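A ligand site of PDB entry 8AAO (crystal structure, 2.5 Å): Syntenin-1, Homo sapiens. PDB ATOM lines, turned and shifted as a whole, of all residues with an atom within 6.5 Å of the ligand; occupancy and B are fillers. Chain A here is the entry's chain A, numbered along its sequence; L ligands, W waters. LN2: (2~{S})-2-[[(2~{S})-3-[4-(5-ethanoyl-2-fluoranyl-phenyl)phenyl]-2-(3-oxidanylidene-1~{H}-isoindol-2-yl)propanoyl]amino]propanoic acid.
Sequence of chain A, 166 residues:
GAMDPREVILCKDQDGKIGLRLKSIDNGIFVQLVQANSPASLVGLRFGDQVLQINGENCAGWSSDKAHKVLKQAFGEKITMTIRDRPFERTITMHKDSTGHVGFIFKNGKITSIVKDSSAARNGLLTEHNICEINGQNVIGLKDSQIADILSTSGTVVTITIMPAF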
ATOM      1  N   LYS A  96      29.674  29.528 -30.587  1.00  0.00           N
ATOM      2  CA  LYS A  96      29.708  28.367 -29.722  1.00  0.00           C
ATOM      3  C   LYS A  96      31.112  28.014 -29.306  1.00  0.00           C
ATOM      4  O   LYS A  96      32.036  28.050 -30.112  1.00  0.00           O
ATOM      5  CB  LYS A  96      29.089  27.170 -30.440  1.00  0.00           C
ATOM      6  CG  LYS A  96      27.581  27.042 -30.299  1.00  0.00           C
ATOM      7  CD  LYS A  96      27.057  26.150 -31.418  1.00  0.00           C
ATOM      8  CE  LYS A  96      25.668  25.631 -31.206  1.00  0.00           C
ATOM      9  NZ  LYS A  96      25.670  24.164 -30.940  1.00  0.00           N
ATOM     10  N   ASP A  97      31.279  27.628 -28.044  1.00  0.00           N
ATOM     11  CA  ASP A  97      32.576  27.190 -27.526  1.00  0.00           C
ATOM     12  C   ASP A  97      32.859  25.694 -27.906  1.00  0.00           C
ATOM     13  O   ASP A  97      32.120  25.106 -28.699  1.00  0.00           O
ATOM     14  CB  ASP A  97      32.652  27.473 -26.009  1.00  0.00           C
ATOM     15  CG  ASP A  97      31.932  26.497 -25.086  1.00  0.00           C
ATOM     16  OD1 ASP A  97      31.036  25.754 -25.567  1.00  0.00           O
ATOM     17  OD2 ASP A  97      32.263  26.467 -23.890  1.00  0.00           O
ATOM     18  N   THR A  99      32.297  23.059 -26.306  1.00  0.00           N
ATOM     19  CA  THR A  99      31.187  22.224 -25.842  1.00  0.00           C
ATOM     20  C   THR A  99      29.850  22.463 -26.587  1.00  0.00           C
ATOM     21  O   THR A  99      28.891  21.743 -26.353  1.00  0.00           O
ATOM     22  CB  THR A  99      30.987  22.389 -24.317  1.00  0.00           C
ATOM     23  OG1 THR A  99      30.315  23.617 -24.034  1.00  0.00           O
ATOM     24  CG2 THR A  99      32.304  22.295 -23.535  1.00  0.00           C
ATOM     25  N   GLY A 100      29.790  23.472 -27.446  1.00  0.00           N
ATOM     26  CA  GLY A 100      28.577  23.796 -28.191  1.00  0.00           C
ATOM     27  C   GLY A 100      27.669  24.779 -27.483  1.00  0.00           C
ATOM     28  O   GLY A 100      26.459  24.793 -27.723  1.00  0.00           O
ATOM     29  N   HIS A 101      28.240  25.629 -26.612  1.00  0.00           N
ATOM     30  CA  HIS A 101      27.422  26.588 -25.874  1.00  0.00           C
ATOM     31  C   HIS A 101      27.844  28.044 -26.046  1.00  0.00           C
ATOM     32  O   HIS A 101      29.015  28.367 -25.878  1.00  0.00           O
ATOM     33  CB  HIS A 101      27.346  26.207 -24.391  1.00  0.00           C
ATOM     34  CG  HIS A 101      26.624  24.921 -24.121  1.00  0.00           C
ATOM     35  ND1 HIS A 101      27.288  23.803 -23.647  1.00  0.00           N
ATOM     36  CD2 HIS A 101      25.309  24.621 -24.248  1.00  0.00           C
ATOM     37  CE1 HIS A 101      26.362  22.862 -23.525  1.00  0.00           C
ATOM     38  NE2 HIS A 101      25.160  23.306 -23.867  1.00  0.00           N
ATOM     39  N   VAL A 102      26.864  28.921 -26.384  1.00  0.00           N
ATOM     40  CA  VAL A 102      27.085  30.372 -26.481  1.00  0.00           C
ATOM     41  C   VAL A 102      27.121  31.003 -25.063  1.00  0.00           C
ATOM     42  O   VAL A 102      27.793  32.002 -24.854  1.00  0.00           O
ATOM     43  CB  VAL A 102      26.090  31.088 -27.441  1.00  0.00           C
ATOM     44  CG1 VAL A 102      26.333  30.662 -28.880  1.00  0.00           C
ATOM     45  CG2 VAL A 102      24.649  30.838 -27.051  1.00  0.00           C
ATOM     46  N   GLY A 103      26.424  30.408 -24.094  1.00  0.00           N
ATOM     47  CA  GLY A 103      26.513  30.832 -22.708  1.00  0.00           C
ATOM     48  C   GLY A 103      25.338  31.508 -22.042  1.00  0.00           C
ATOM     49  O   GLY A 103      25.555  32.393 -21.219  1.00  0.00           O
ATOM     50  N   PHE A 104      24.106  31.094 -22.346  1.00  0.00           N
ATOM     51  CA  PHE A 104      22.944  31.658 -21.652  1.00  0.00           C
ATOM     52  C   PHE A 104      21.922  30.592 -21.280  1.00  0.00           C
ATOM     53  O   PHE A 104      22.009  29.458 -21.721  1.00  0.00           O
ATOM     54  CB  PHE A 104      22.312  32.844 -22.424  1.00  0.00           C
ATOM     55  CG  PHE A 104      21.591  32.520 -23.716  1.00  0.00           C
ATOM     56  CD1 PHE A 104      20.263  32.126 -23.709  1.00  0.00           C
ATOM     57  CD2 PHE A 104      22.218  32.663 -24.936  1.00  0.00           C
ATOM     58  CE1 PHE A 104      19.594  31.863 -24.897  1.00  0.00           C
ATOM     59  CE2 PHE A 104      21.530  32.448 -26.108  1.00  0.00           C
ATOM     60  CZ  PHE A 104      20.224  32.045 -26.084  1.00  0.00           C
ATOM     61  N   ILE A 105      20.972  30.952 -20.404  1.00  0.00           N
ATOM     62  CA  ILE A 105      19.902  30.071 -19.946  1.00  0.00           C
ATOM     63  C   ILE A 105      18.595  30.759 -20.303  1.00  0.00           C
ATOM     64  O   ILE A 105      18.468  31.960 -20.104  1.00  0.00           O
ATOM     65  CB  ILE A 105      20.028  29.878 -18.416  1.00  0.00           C
ATOM     66  CG1 ILE A 105      21.320  29.144 -18.043  1.00  0.00           C
ATOM     67  CG2 ILE A 105      18.796  29.203 -17.797  1.00  0.00           C
ATOM     68  CD1 ILE A 105      21.401  27.799 -18.551  1.00  0.00           C
ATOM     69  N   PHE A 106      17.635  30.032 -20.876  1.00  0.00           N
ATOM     70  CA  PHE A 106      16.338  30.617 -21.183  1.00  0.00           C
ATOM     71  C   PHE A 106      15.182  29.837 -20.527  1.00  0.00           C
ATOM     72  O   PHE A 106      15.337  28.671 -20.184  1.00  0.00           O
ATOM     73  CB  PHE A 106      16.129  30.826 -22.693  1.00  0.00           C
ATOM     74  CG  PHE A 106      16.218  29.558 -23.501  1.00  0.00           C
ATOM     75  CD1 PHE A 106      17.442  29.098 -23.965  1.00  0.00           C
ATOM     76  CD2 PHE A 106      15.084  28.846 -23.838  1.00  0.00           C
ATOM     77  CE1 PHE A 106      17.519  27.931 -24.710  1.00  0.00           C
ATOM     78  CE2 PHE A 106      15.166  27.682 -24.574  1.00  0.00           C
ATOM     79  CZ  PHE A 106      16.386  27.233 -25.003  1.00  0.00           C
ATOM     80  N   LYS A 107      14.069  30.517 -20.275  1.00  0.00           N
ATOM     81  CA  LYS A 107      12.855  29.939 -19.697  1.00  0.00           C
ATOM     82  C   LYS A 107      11.684  30.731 -20.243  1.00  0.00           C
ATOM     83  O   LYS A 107      11.565  31.927 -19.973  1.00  0.00           O
ATOM     84  CB  LYS A 107      12.880  29.980 -18.169  1.00  0.00           C
ATOM     85  CG  LYS A 107      11.610  29.375 -17.556  1.00  0.00           C
ATOM     86  CD  LYS A 107      11.851  28.065 -16.792  1.00  0.00           C
ATOM     87  CE  LYS A 107      12.623  28.267 -15.503  1.00  0.00           C
ATOM     88  NZ  LYS A 107      12.704  27.030 -14.659  1.00  0.00           N
ATOM     89  N   THR A 112      17.329  34.244 -19.039  1.00  0.00           N
ATOM     90  CA  THR A 112      17.275  34.460 -17.600  1.00  0.00           C
ATOM     91  C   THR A 112      18.669  34.648 -16.986  1.00  0.00           C
ATOM     92  O   THR A 112      18.806  35.382 -15.999  1.00  0.00           O
ATOM     93  CB  THR A 112      16.472  33.353 -16.883  1.00  0.00           C
ATOM     94  OG1 THR A 112      17.101  32.085 -17.061  1.00  0.00           O
ATOM     95  CG2 THR A 112      15.029  33.326 -17.312  1.00  0.00           C
ATOM     96  N   VAL A 115      26.210  32.913 -18.534  1.00  0.00           N
ATOM     97  CA  VAL A 115      27.310  32.157 -17.971  1.00  0.00           C
ATOM     98  C   VAL A 115      28.555  33.040 -17.951  1.00  0.00           C
ATOM     99  O   VAL A 115      28.860  33.693 -18.942  1.00  0.00           O
ATOM    100  CB  VAL A 115      27.547  30.833 -18.759  1.00  0.00           C
ATOM    101  CG1 VAL A 115      28.708  30.046 -18.170  1.00  0.00           C
ATOM    102  CG2 VAL A 115      26.281  29.984 -18.793  1.00  0.00           C
ATOM    103  N   LYS A 116      29.250  33.090 -16.812  1.00  0.00           N
ATOM    104  CA  LYS A 116      30.476  33.876 -16.701  1.00  0.00           C
ATOM    105  C   LYS A 116      31.553  33.300 -17.650  1.00  0.00           C
ATOM    106  O   LYS A 116      31.659  32.072 -17.774  1.00  0.00           O
ATOM    107  CB  LYS A 116      30.986  33.837 -15.249  1.00  0.00           C
ATOM    108  CG  LYS A 116      31.924  34.973 -14.875  1.00  0.00           C
ATOM    109  CD  LYS A 116      32.731  34.603 -13.611  1.00  0.00           C
ATOM    110  CE  LYS A 116      33.668  33.438 -13.822  1.00  0.00           C
ATOM    111  NZ  LYS A 116      35.003  33.857 -14.320  1.00  0.00           N
ATOM    112  N   ASP A 117      32.315  34.209 -18.344  1.00  0.00           N
ATOM    113  CA  ASP A 117      33.413  33.915 -19.289  1.00  0.00           C
ATOM    114  C   ASP A 117      32.934  33.162 -20.521  1.00  0.00           C
ATOM    115  O   ASP A 117      33.546  32.184 -20.950  1.00  0.00           O
ATOM    116  CB  ASP A 117      34.624  33.200 -18.625  1.00  0.00           C
ATOM    117  CG  ASP A 117      35.368  34.048 -17.597  1.00  0.00           C
ATOM    118  OD1 ASP A 117      35.242  35.309 -17.637  1.00  0.00           O
ATOM    119  OD2 ASP A 117      36.111  33.449 -16.745  1.00  0.00           O
ATOM    120  N   SER A 118      31.849  33.648 -21.102  1.00  0.00           N
ATOM    121  CA  SER A 118      31.233  33.009 -22.248  1.00  0.00           C
ATOM    122  C   SER A 118      31.071  33.969 -23.423  1.00  0.00           C
ATOM    123  O   SER A 118      31.275  35.180 -23.269  1.00  0.00           O
ATOM    124  CB  SER A 118      29.893  32.428 -21.828  1.00  0.00           C
ATOM    125  OG  SER A 118      28.998  33.454 -21.409  1.00  0.00           O
ATOM    126  N   SER A 119      30.701  33.438 -24.617  1.00  0.00           N
ATOM    127  CA  SER A 119      30.449  34.264 -25.791  1.00  0.00           C
ATOM    128  C   SER A 119      29.269  35.201 -25.571  1.00  0.00           C
ATOM    129  O   SER A 119      29.298  36.335 -26.051  1.00  0.00           O
ATOM    130  CB  SER A 119      30.176  33.399 -27.013  1.00  0.00           C
ATOM    131  OG  SER A 119      30.246  34.179 -28.202  1.00  0.00           O
ATOM    132  N   ALA A 120      28.240  34.752 -24.824  1.00  0.00           N
ATOM    133  CA  ALA A 120      27.085  35.598 -24.493  1.00  0.00           C
ATOM    134  C   ALA A 120      27.549  36.738 -23.605  1.00  0.00           C
ATOM    135  O   ALA A 120      27.076  37.868 -23.776  1.00  0.00           O
ATOM    136  CB  ALA A 120      26.014  34.792 -23.778  1.00  0.00           C
ATOM    137  N   ASP A 144      10.320  25.902 -25.326  1.00  0.00           N
ATOM    138  CA  ASP A 144      11.756  25.886 -25.037  1.00  0.00           C
ATOM    139  C   ASP A 144      12.486  24.684 -25.655  1.00  0.00           C
ATOM    140  O   ASP A 144      13.555  24.859 -26.246  1.00  0.00           O
ATOM    141  CB  ASP A 144      11.989  25.985 -23.536  1.00  0.00           C
ATOM    142  CG  ASP A 144      11.532  27.314 -22.954  1.00  0.00           C
ATOM    143  OD1 ASP A 144      11.494  28.327 -23.702  1.00  0.00           O
ATOM    144  OD2 ASP A 144      11.216  27.361 -21.732  1.00  0.00           O
ATOM    145  N   SER A 145      11.872  23.508 -25.635  1.00  0.00           N
ATOM    146  CA  SER A 145      12.472  22.314 -26.239  1.00  0.00           C
ATOM    147  C   SER A 145      12.732  22.519 -27.735  1.00  0.00           C
ATOM    148  O   SER A 145      13.773  22.103 -28.218  1.00  0.00           O
ATOM    149  CB  SER A 145      11.556  21.113 -26.036  1.00  0.00           C
ATOM    150  OG  SER A 145      10.238  21.440 -26.444  1.00  0.00           O
ATOM    151  N   ALA A 148      15.681  24.986 -28.177  1.00  0.00           N
ATOM    152  CA  ALA A 148      16.936  24.286 -27.920  1.00  0.00           C
ATOM    153  C   ALA A 148      17.342  23.391 -29.082  1.00  0.00           C
ATOM    154  O   ALA A 148      18.536  23.217 -29.314  1.00  0.00           O
ATOM    155  CB  ALA A 148      16.815  23.472 -26.647  1.00  0.00           C
ATOM    156  N   LEU A 151      19.083  25.569 -31.645  1.00  0.00           N
ATOM    157  CA  LEU A 151      20.425  25.831 -31.118  1.00  0.00           C
ATOM    158  C   LEU A 151      21.351  24.622 -31.241  1.00  0.00           C
ATOM    159  O   LEU A 151      22.548  24.776 -31.539  1.00  0.00           O
ATOM    160  CB  LEU A 151      20.313  26.250 -29.656  1.00  0.00           C
ATOM    161  CG  LEU A 151      19.692  27.608 -29.485  1.00  0.00           C
ATOM    162  CD1 LEU A 151      19.169  27.792 -28.120  1.00  0.00           C
ATOM    163  CD2 LEU A 151      20.661  28.674 -29.899  1.00  0.00           C
ATOM    164  N   VAL A 158      25.944  31.850 -33.859  1.00  0.00           N
ATOM    165  CA  VAL A 158      24.541  31.931 -33.460  1.00  0.00           C
ATOM    166  C   VAL A 158      24.187  33.400 -33.361  1.00  0.00           C
ATOM    167  O   VAL A 158      24.678  34.098 -32.476  1.00  0.00           O
ATOM    168  CB  VAL A 158      24.325  31.233 -32.104  1.00  0.00           C
ATOM    169  CG1 VAL A 158      22.861  31.333 -31.675  1.00  0.00           C
ATOM    170  CG2 VAL A 158      24.802  29.788 -32.150  1.00  0.00           C
ATOM    171  N   ILE A 160      21.265  36.092 -32.654  1.00  0.00           N
ATOM    172  CA  ILE A 160      19.940  36.155 -32.033  1.00  0.00           C
ATOM    173  C   ILE A 160      19.335  37.547 -31.986  1.00  0.00           C
ATOM    174  O   ILE A 160      19.961  38.469 -31.466  1.00  0.00           O
ATOM    175  CB  ILE A 160      19.996  35.499 -30.612  1.00  0.00           C
ATOM    176  CG1 ILE A 160      20.264  33.983 -30.724  1.00  0.00           C
ATOM    177  CG2 ILE A 160      18.733  35.764 -29.803  1.00  0.00           C
ATOM    178  CD1 ILE A 160      20.273  33.220 -29.453  1.00  0.00           C
HETATM  179  O1  LN2 L   1      21.871  25.131 -24.036  1.00  0.00           O
HETATM  180  O2  LN2 L   1      24.328  27.284 -25.977  1.00  0.00           O
HETATM  181  O3  LN2 L   1      23.952  28.677 -24.273  1.00  0.00           O
HETATM  182  O4  LN2 L   1      18.698  27.207 -20.714  1.00  0.00           O
HETATM  183  C1  LN2 L   1      30.000  28.517 -21.887  1.00  0.00           C
HETATM  184  C2  LN2 L   1      29.360  27.499 -21.008  1.00  0.00           C
HETATM  185  O   LN2 L   1      29.376  29.003 -22.812  1.00  0.00           O
HETATM  186  C24 LN2 L   1      18.541  26.267 -21.462  1.00  0.00           C
HETATM  187  C23 LN2 L   1      17.291  25.548 -21.799  1.00  0.00           C
HETATM  188  C22 LN2 L   1      15.980  25.753 -21.372  1.00  0.00           C
HETATM  189  C21 LN2 L   1      14.989  24.860 -21.756  1.00  0.00           C
HETATM  190  C20 LN2 L   1      15.297  23.791 -22.572  1.00  0.00           C
HETATM  191  C19 LN2 L   1      16.592  23.599 -23.007  1.00  0.00           C
HETATM  192  C18 LN2 L   1      17.595  24.476 -22.624  1.00  0.00           C
HETATM  193  C17 LN2 L   1      19.067  24.481 -22.915  1.00  0.00           C
HETATM  194  N1  LN2 L   1      19.536  25.612 -22.127  1.00  0.00           N
HETATM  195  C12 LN2 L   1      20.931  26.016 -22.018  1.00  0.00           C
HETATM  196  C13 LN2 L   1      21.483  26.119 -23.436  1.00  0.00           C
HETATM  197  N   LN2 L   1      21.514  27.351 -23.959  1.00  0.00           N
HETATM  198  C14 LN2 L   1      22.072  27.605 -25.271  1.00  0.00           C
HETATM  199  C16 LN2 L   1      23.573  27.827 -25.199  1.00  0.00           C
HETATM  200  C15 LN2 L   1      21.423  28.829 -25.899  1.00  0.00           C
HETATM  201  C11 LN2 L   1      21.759  25.039 -21.156  1.00  0.00           C
HETATM  202  C10 LN2 L   1      23.221  25.392 -20.979  1.00  0.00           C
HETATM  203  C9  LN2 L   1      23.629  26.695 -20.764  1.00  0.00           C
HETATM  204  C8  LN2 L   1      24.954  27.003 -20.521  1.00  0.00           C
HETATM  205  C25 LN2 L   1      24.186  24.393 -20.966  1.00  0.00           C
HETATM  206  C26 LN2 L   1      25.511  24.701 -20.723  1.00  0.00           C
HETATM  207  C7  LN2 L   1      25.929  26.011 -20.492  1.00  0.00           C
HETATM  208  C6  LN2 L   1      27.361  26.344 -20.263  1.00  0.00           C
HETATM  209  C5  LN2 L   1      28.144  25.677 -19.332  1.00  0.00           C
HETATM  210  F   LN2 L   1      27.562  24.796 -18.486  1.00  0.00           F
HETATM  211  C4  LN2 L   1      29.501  25.873 -19.223  1.00  0.00           C
HETATM  212  C3  LN2 L   1      30.107  26.782 -20.072  1.00  0.00           C
HETATM  213  C27 LN2 L   1      27.988  27.269 -21.094  1.00  0.00           C
HETATM  214  C   LN2 L   1      31.410  28.945 -21.610  1.00  0.00           C
HETATM  215  O   HOH W   1      30.442  30.403 -24.903  1.00  0.00           O
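The backbone NH (N) of Val 115 is in hydrogen-bond range of the backbone carbonyl oxygen (O) of Gly 103, at 2.8 Å.
The backbone carbonyl oxygen of Val 102 lies within hydrogen-bond range of the backbone NH of Ala 120 (2.8 Å).
The backbone NH (N) of His 101 sits at hydrogen-bond distance from the side-chain carboxylate (OD1) of Asp 97 (3.0 Å).
A ring nitrogen (ND1) of His 101 is in hydrogen-bond range of the side-chain hydroxyl (OG1) of Thr 99.
O of Ile 105 is in hydrogen-bond range of N of Thr 112 (2.8 Å).
The side-chain carboxylate of Asp 97 sits at hydrogen-bond distance from the backbone NH of Gly 100, at 3.2 Å.
The side-chain hydroxyl (OG) of Ser 118 is in hydrogen-bond range of the backbone carbonyl oxygen (O) of Val 115 (2.5 Å).
The backbone carbonyl oxygen of Gly 100 is in hydrogen-bond range of the side-chain amino group of Lys 96, at 3.4 Å.
The backbone NH of Phe 106 is in hydrogen-bond range of an oxygen (O4) of the ligand, 3.0 Å away.
N of Gly 103 lies within hydrogen-bond range of O3 of the ligand, at 3.0 Å.
O2 of the ligand is in hydrogen-bond range of N of Val 102.
N of Phe 104 sits at hydrogen-bond distance from O3 of the ligand (3.1 Å).
The backbone carbonyl oxygen (O) of Phe 104 sits at hydrogen-bond distance from a nitrogen (N) of the ligand.
The backbone carbonyl oxygen of His 101 lies close to an oxygen (O) of the ligand (3.2 Å).
Merely in contact with the ligand: Ile 105 (3.2 Å), Leu 151 (3.3 Å), Asp 97 (3.5 Å), Ser 118 (3.6 Å), Ala 148 (3.6 Å), Asp 144 (3.7 Å), Val 115 (3.7 Å), Gly 100 (3.7 Å) and Asp 117 (3.9 Å).
The nearest printed residue that does not touch the ligand is Ser 145 (4.6 Å).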
